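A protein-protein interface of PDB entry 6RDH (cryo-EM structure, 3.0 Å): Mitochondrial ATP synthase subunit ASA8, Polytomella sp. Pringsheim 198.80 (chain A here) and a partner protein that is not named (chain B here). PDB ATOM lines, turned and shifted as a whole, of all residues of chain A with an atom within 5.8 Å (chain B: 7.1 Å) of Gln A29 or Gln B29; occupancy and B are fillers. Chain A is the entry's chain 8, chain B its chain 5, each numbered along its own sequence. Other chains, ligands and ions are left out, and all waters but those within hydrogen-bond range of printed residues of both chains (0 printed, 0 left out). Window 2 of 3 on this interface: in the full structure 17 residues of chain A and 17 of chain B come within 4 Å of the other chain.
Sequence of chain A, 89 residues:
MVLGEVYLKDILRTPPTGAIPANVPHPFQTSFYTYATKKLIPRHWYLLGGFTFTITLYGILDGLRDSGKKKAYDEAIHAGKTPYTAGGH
NE2 of Gln B29 lies within hydrogen-bond range of OE1 of Gln A29 (3.2 Å).
The backbone carbonyl oxygen of Val A24 lies within hydrogen-bond range of the guanidinium group of Arg B36.
The backbone carbonyl oxygen of Trp B24 sits close to the side-chain hydroxyl of Thr B28 (3.2 Å).
The backbone carbonyl oxygen (O) of Gln B29 is in hydrogen-bond range of the side-chain hydroxyl (OG1) of Thr B33 (2.9 Å).
Among the printed residues, merely in contact across the chains: Phe A28 with Thr B28 (3.4 Å), Gln A29 with Thr B28 (3.5 Å), His A26 with Pro B32 (3.7 Å), Phe A28 with Asp B27 (3.8 Å), His A26 with Arg B36 (3.8 Å) and Pro A25 with Arg B36 (3.9 Å).
Gln A29 touches just these residues of chain B: Thr B28 (3.5 Å) and Gln B29 (3.2 Å).
Printed residues of chain A within 4 Å of Thr B28: Phe A28 (3.4 Å) and Gln A29 (3.5 Å).
Printed residues of chain B within 4 Å of Phe A28: Asp B27 (3.8 Å) and Thr B28 (3.4 Å).
Of the printed residues of chain A, Pro B32 touches His A26.
Printed residues of chain B within 4 Å of Val A24: Arg B36 (2.8 Å).
Of the printed residues of chain B, His A26 touches Pro B32 and Arg B36.
Trp B24 touches none of the printed residues of chain A.
The nearest residue of chain B that does not touch Gln A29 is Pro B32 (4.3 Å).
The nearest printed residue of chain A that does not touch Pro B32 is Gln A29 (4.3 Å).
Among the printed residues, 8 pairs touch across the chains.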
ATOM      1  N   VAL A  24      27.964  14.591 -16.031  1.00  0.00           N
ATOM      2  CA  VAL A  24      27.545  14.826 -14.655  1.00  0.00           C
ATOM      3  C   VAL A  24      26.836  13.582 -14.144  1.00  0.00           C
ATOM      4  O   VAL A  24      25.838  13.152 -14.738  1.00  0.00           O
ATOM      5  CB  VAL A  24      26.633  16.051 -14.552  1.00  0.00           C
ATOM      6  CG1 VAL A  24      26.017  16.128 -13.191  1.00  0.00           C
ATOM      7  CG2 VAL A  24      27.410  17.288 -14.826  1.00  0.00           C
ATOM      8  N   PRO A  25      27.308  12.963 -13.072  1.00  0.00           N
ATOM      9  CA  PRO A  25      26.668  11.746 -12.594  1.00  0.00           C
ATOM     10  C   PRO A  25      25.363  12.037 -11.886  1.00  0.00           C
ATOM     11  O   PRO A  25      25.218  13.031 -11.174  1.00  0.00           O
ATOM     12  CB  PRO A  25      27.693  11.173 -11.611  1.00  0.00           C
ATOM     13  CG  PRO A  25      28.916  11.931 -11.827  1.00  0.00           C
ATOM     14  CD  PRO A  25      28.512  13.265 -12.296  1.00  0.00           C
ATOM     15  N   HIS A  26      24.407  11.149 -12.104  1.00  0.00           N
ATOM     16  CA  HIS A  26      23.220  11.121 -11.281  1.00  0.00           C
ATOM     17  C   HIS A  26      23.610  10.741  -9.856  1.00  0.00           C
ATOM     18  O   HIS A  26      24.608  10.049  -9.653  1.00  0.00           O
ATOM     19  CB  HIS A  26      22.227  10.118 -11.847  1.00  0.00           C
ATOM     20  CG  HIS A  26      20.884  10.173 -11.205  1.00  0.00           C
ATOM     21  ND1 HIS A  26      20.051  11.254 -11.326  1.00  0.00           N
ATOM     22  CD2 HIS A  26      20.241   9.291 -10.412  1.00  0.00           C
ATOM     23  CE1 HIS A  26      18.949  11.037 -10.637  1.00  0.00           C
ATOM     24  NE2 HIS A  26      19.037   9.851 -10.075  1.00  0.00           N
ATOM     25  N   PRO A  27      22.863  11.201  -8.848  1.00  0.00           N
ATOM     26  CA  PRO A  27      23.156  10.787  -7.467  1.00  0.00           C
ATOM     27  C   PRO A  27      23.044   9.295  -7.194  1.00  0.00           C
ATOM     28  O   PRO A  27      23.556   8.841  -6.170  1.00  0.00           O
ATOM     29  CB  PRO A  27      22.124  11.566  -6.657  1.00  0.00           C
ATOM     30  CG  PRO A  27      21.918  12.780  -7.430  1.00  0.00           C
ATOM     31  CD  PRO A  27      22.040  12.420  -8.868  1.00  0.00           C
ATOM     32  N   PHE A  28      22.389   8.519  -8.055  1.00  0.00           N
ATOM     33  CA  PHE A  28      22.390   7.076  -7.889  1.00  0.00           C
ATOM     34  C   PHE A  28      23.644   6.452  -8.461  1.00  0.00           C
ATOM     35  O   PHE A  28      24.039   5.368  -8.033  1.00  0.00           O
ATOM     36  CB  PHE A  28      21.185   6.443  -8.569  1.00  0.00           C
ATOM     37  CG  PHE A  28      19.873   6.832  -7.985  1.00  0.00           C
ATOM     38  CD1 PHE A  28      19.771   7.291  -6.693  1.00  0.00           C
ATOM     39  CD2 PHE A  28      18.734   6.731  -8.735  1.00  0.00           C
ATOM     40  CE1 PHE A  28      18.567   7.649  -6.177  1.00  0.00           C
ATOM     41  CE2 PHE A  28      17.539   7.084  -8.214  1.00  0.00           C
ATOM     42  CZ  PHE A  28      17.457   7.537  -6.932  1.00  0.00           C
ATOM     43  N   GLN A  29      24.267   7.094  -9.439  1.00  0.00           N
ATOM     44  CA  GLN A  29      25.467   6.535 -10.033  1.00  0.00           C
ATOM     45  C   GLN A  29      26.692   6.737  -9.167  1.00  0.00           C
ATOM     46  O   GLN A  29      27.678   6.019  -9.341  1.00  0.00           O
ATOM     47  CB  GLN A  29      25.729   7.152 -11.400  1.00  0.00           C
ATOM     48  CG  GLN A  29      24.566   7.120 -12.339  1.00  0.00           C
ATOM     49  CD  GLN A  29      24.998   7.354 -13.749  1.00  0.00           C
ATOM     50  OE1 GLN A  29      26.068   6.924 -14.150  1.00  0.00           O
ATOM     51  NE2 GLN A  29      24.174   8.046 -14.516  1.00  0.00           N
ATOM     52  N   THR A  30      26.666   7.704  -8.256  1.00  0.00           N
ATOM     53  CA  THR A  30      27.810   7.903  -7.378  1.00  0.00           C
ATOM     54  C   THR A  30      27.762   6.955  -6.192  1.00  0.00           C
ATOM     55  O   THR A  30      28.637   6.102  -6.032  1.00  0.00           O
ATOM     56  CB  THR A  30      27.867   9.346  -6.897  1.00  0.00           C
ATOM     57  OG1 THR A  30      26.594   9.720  -6.367  1.00  0.00           O
ATOM     58  CG2 THR A  30      28.213  10.252  -8.043  1.00  0.00           C
ATOM     59  N   SER A  31      26.740   7.075  -5.358  1.00  0.00           N
ATOM     60  CA  SER A  31      26.682   6.330  -4.113  1.00  0.00           C
ATOM     61  C   SER A  31      25.525   5.352  -4.139  1.00  0.00           C
ATOM     62  O   SER A  31      24.405   5.720  -4.498  1.00  0.00           O
ATOM     63  CB  SER A  31      26.528   7.266  -2.920  1.00  0.00           C
ATOM     64  OG  SER A  31      25.210   7.755  -2.869  1.00  0.00           O
ATOM     65  N   LEU B  23      17.460  -4.775 -12.098  1.00  0.00           N
ATOM     66  CA  LEU B  23      16.701  -3.676 -11.515  1.00  0.00           C
ATOM     67  C   LEU B  23      17.602  -2.528 -11.095  1.00  0.00           C
ATOM     68  O   LEU B  23      17.284  -1.367 -11.363  1.00  0.00           O
ATOM     69  CB  LEU B  23      15.906  -4.173 -10.321  1.00  0.00           C
ATOM     70  CG  LEU B  23      15.157  -3.115  -9.545  1.00  0.00           C
ATOM     71  CD1 LEU B  23      14.095  -2.551 -10.420  1.00  0.00           C
ATOM     72  CD2 LEU B  23      14.563  -3.746  -8.333  1.00  0.00           C
ATOM     73  N   TRP B  24      18.729  -2.827 -10.447  1.00  0.00           N
ATOM     74  CA  TRP B  24      19.655  -1.770 -10.054  1.00  0.00           C
ATOM     75  C   TRP B  24      20.251  -1.083 -11.269  1.00  0.00           C
ATOM     76  O   TRP B  24      20.364   0.141 -11.293  1.00  0.00           O
ATOM     77  CB  TRP B  24      20.777  -2.319  -9.175  1.00  0.00           C
ATOM     78  CG  TRP B  24      21.932  -1.369  -9.028  1.00  0.00           C
ATOM     79  CD1 TRP B  24      22.049  -0.370  -8.125  1.00  0.00           C
ATOM     80  CD2 TRP B  24      23.129  -1.337  -9.812  1.00  0.00           C
ATOM     81  NE1 TRP B  24      23.236   0.292  -8.296  1.00  0.00           N
ATOM     82  CE2 TRP B  24      23.913  -0.284  -9.334  1.00  0.00           C
ATOM     83  CE3 TRP B  24      23.602  -2.091 -10.880  1.00  0.00           C
ATOM     84  CZ2 TRP B  24      25.141   0.025  -9.881  1.00  0.00           C
ATOM     85  CZ3 TRP B  24      24.806  -1.779 -11.423  1.00  0.00           C
ATOM     86  CH2 TRP B  24      25.570  -0.737 -10.923  1.00  0.00           C
ATOM     87  N   HIS B  25      20.626  -1.851 -12.290  1.00  0.00           N
ATOM     88  CA  HIS B  25      21.297  -1.268 -13.438  1.00  0.00           C
ATOM     89  C   HIS B  25      20.347  -0.437 -14.259  1.00  0.00           C
ATOM     90  O   HIS B  25      20.720   0.642 -14.709  1.00  0.00           O
ATOM     91  CB  HIS B  25      21.920  -2.345 -14.300  1.00  0.00           C
ATOM     92  CG  HIS B  25      22.801  -1.803 -15.372  1.00  0.00           C
ATOM     93  ND1 HIS B  25      22.404  -1.711 -16.684  1.00  0.00           N
ATOM     94  CD2 HIS B  25      24.052  -1.296 -15.322  1.00  0.00           C
ATOM     95  CE1 HIS B  25      23.378  -1.184 -17.400  1.00  0.00           C
ATOM     96  NE2 HIS B  25      24.389  -0.923 -16.595  1.00  0.00           N
ATOM     97  N   LEU B  26      19.115  -0.905 -14.417  1.00  0.00           N
ATOM     98  CA  LEU B  26      18.046  -0.100 -14.985  1.00  0.00           C
ATOM     99  C   LEU B  26      17.885   1.202 -14.224  1.00  0.00           C
ATOM    100  O   LEU B  26      18.284   2.261 -14.714  1.00  0.00           O
ATOM    101  CB  LEU B  26      16.765  -0.903 -14.930  1.00  0.00           C
ATOM    102  CG  LEU B  26      15.516  -0.348 -15.547  1.00  0.00           C
ATOM    103  CD1 LEU B  26      15.631  -0.379 -17.036  1.00  0.00           C
ATOM    104  CD2 LEU B  26      14.449  -1.231 -15.072  1.00  0.00           C
ATOM    105  N   ASP B  27      17.484   1.097 -12.959  1.00  0.00           N
ATOM    106  CA  ASP B  27      17.108   2.219 -12.117  1.00  0.00           C
ATOM    107  C   ASP B  27      18.231   3.207 -11.868  1.00  0.00           C
ATOM    108  O   ASP B  27      17.958   4.370 -11.574  1.00  0.00           O
ATOM    109  CB  ASP B  27      16.641   1.652 -10.800  1.00  0.00           C
ATOM    110  CG  ASP B  27      15.514   2.404 -10.222  1.00  0.00           C
ATOM    111  OD1 ASP B  27      15.085   3.391 -10.846  1.00  0.00           O
ATOM    112  OD2 ASP B  27      15.043   1.992  -9.151  1.00  0.00           O
ATOM    113  N   THR B  28      19.477   2.782 -11.983  1.00  0.00           N
ATOM    114  CA  THR B  28      20.624   3.602 -11.655  1.00  0.00           C
ATOM    115  C   THR B  28      21.390   4.072 -12.878  1.00  0.00           C
ATOM    116  O   THR B  28      21.685   5.260 -13.000  1.00  0.00           O
ATOM    117  CB  THR B  28      21.526   2.797 -10.728  1.00  0.00           C
ATOM    118  OG1 THR B  28      20.903   2.706  -9.452  1.00  0.00           O
ATOM    119  CG2 THR B  28      22.838   3.439 -10.559  1.00  0.00           C
ATOM    120  N   GLN B  29      21.720   3.184 -13.806  1.00  0.00           N
ATOM    121  CA  GLN B  29      22.514   3.571 -14.948  1.00  0.00           C
ATOM    122  C   GLN B  29      21.698   3.821 -16.197  1.00  0.00           C
ATOM    123  O   GLN B  29      22.078   4.681 -16.991  1.00  0.00           O
ATOM    124  CB  GLN B  29      23.554   2.496 -15.233  1.00  0.00           C
ATOM    125  CG  GLN B  29      24.246   2.001 -14.002  1.00  0.00           C
ATOM    126  CD  GLN B  29      25.299   2.944 -13.525  1.00  0.00           C
ATOM    127  OE1 GLN B  29      25.606   3.000 -12.343  1.00  0.00           O
ATOM    128  NE2 GLN B  29      25.869   3.701 -14.445  1.00  0.00           N
ATOM    129  N   LEU B  30      20.593   3.109 -16.413  1.00  0.00           N
ATOM    130  CA  LEU B  30      19.897   3.293 -17.675  1.00  0.00           C
ATOM    131  C   LEU B  30      18.806   4.339 -17.565  1.00  0.00           C
ATOM    132  O   LEU B  30      18.754   5.243 -18.391  1.00  0.00           O
ATOM    133  CB  LEU B  30      19.308   1.972 -18.157  1.00  0.00           C
ATOM    134  CG  LEU B  30      20.282   0.894 -18.605  1.00  0.00           C
ATOM    135  CD1 LEU B  30      19.519  -0.348 -18.929  1.00  0.00           C
ATOM    136  CD2 LEU B  30      21.054   1.352 -19.801  1.00  0.00           C
ATOM    137  N   LEU B  31      17.954   4.250 -16.546  1.00  0.00           N
ATOM    138  CA  LEU B  31      16.827   5.170 -16.438  1.00  0.00           C
ATOM    139  C   LEU B  31      17.192   6.637 -16.212  1.00  0.00           C
ATOM    140  O   LEU B  31      16.429   7.489 -16.695  1.00  0.00           O
ATOM    141  CB  LEU B  31      15.869   4.689 -15.342  1.00  0.00           C
ATOM    142  CG  LEU B  31      14.582   4.003 -15.771  1.00  0.00           C
ATOM    143  CD1 LEU B  31      13.709   3.787 -14.569  1.00  0.00           C
ATOM    144  CD2 LEU B  31      13.886   4.857 -16.781  1.00  0.00           C
ATOM    145  N   PRO B  32      18.271   7.013 -15.511  1.00  0.00           N
ATOM    146  CA  PRO B  32      18.734   8.401 -15.633  1.00  0.00           C
ATOM    147  C   PRO B  32      19.126   8.804 -17.036  1.00  0.00           C
ATOM    148  O   PRO B  32      18.796   9.909 -17.465  1.00  0.00           O
ATOM    149  CB  PRO B  32      19.928   8.426 -14.688  1.00  0.00           C
ATOM    150  CG  PRO B  32      19.502   7.575 -13.633  1.00  0.00           C
ATOM    151  CD  PRO B  32      18.827   6.427 -14.282  1.00  0.00           C
ATOM    152  N   THR B  33      19.786   7.926 -17.777  1.00  0.00           N
ATOM    153  CA  THR B  33      20.198   8.246 -19.137  1.00  0.00           C
ATOM    154  C   THR B  33      19.013   8.269 -20.092  1.00  0.00           C
ATOM    155  O   THR B  33      18.979   9.086 -21.013  1.00  0.00           O
ATOM    156  CB  THR B  33      21.234   7.233 -19.584  1.00  0.00           C
ATOM    157  OG1 THR B  33      22.241   7.130 -18.574  1.00  0.00           O
ATOM    158  CG2 THR B  33      21.866   7.655 -20.843  1.00  0.00           C
ATOM    159  N   ILE B  34      18.048   7.362 -19.900  1.00  0.00           N
ATOM    160  CA  ILE B  34      16.787   7.419 -20.634  1.00  0.00           C
ATOM    161  C   ILE B  34      16.098   8.743 -20.372  1.00  0.00           C
ATOM    162  O   ILE B  34      15.698   9.449 -21.299  1.00  0.00           O
ATOM    163  CB  ILE B  34      15.858   6.256 -20.232  1.00  0.00           C
ATOM    164  CG1 ILE B  34      16.435   4.879 -20.522  1.00  0.00           C
ATOM    165  CG2 ILE B  34      14.534   6.381 -20.918  1.00  0.00           C
ATOM    166  CD1 ILE B  34      16.733   4.613 -21.897  1.00  0.00           C
ATOM    167  N   ARG B  36      17.081  11.670 -19.026  1.00  0.00           N
ATOM    168  CA  ARG B  36      17.716  12.932 -19.378  1.00  0.00           C
ATOM    169  C   ARG B  36      17.412  13.316 -20.813  1.00  0.00           C
ATOM    170  O   ARG B  36      16.929  14.420 -21.084  1.00  0.00           O
ATOM    171  CB  ARG B  36      19.216  12.836 -19.176  1.00  0.00           C
ATOM    172  CG  ARG B  36      19.648  13.100 -17.786  1.00  0.00           C
ATOM    173  CD  ARG B  36      21.120  12.982 -17.680  1.00  0.00           C
ATOM    174  NE  ARG B  36      21.535  13.238 -16.318  1.00  0.00           N
ATOM    175  CZ  ARG B  36      22.795  13.346 -15.942  1.00  0.00           C
ATOM    176  NH1 ARG B  36      23.086  13.589 -14.677  1.00  0.00           N
ATOM    177  NH2 ARG B  36      23.759  13.209 -16.831  1.00  0.00           N
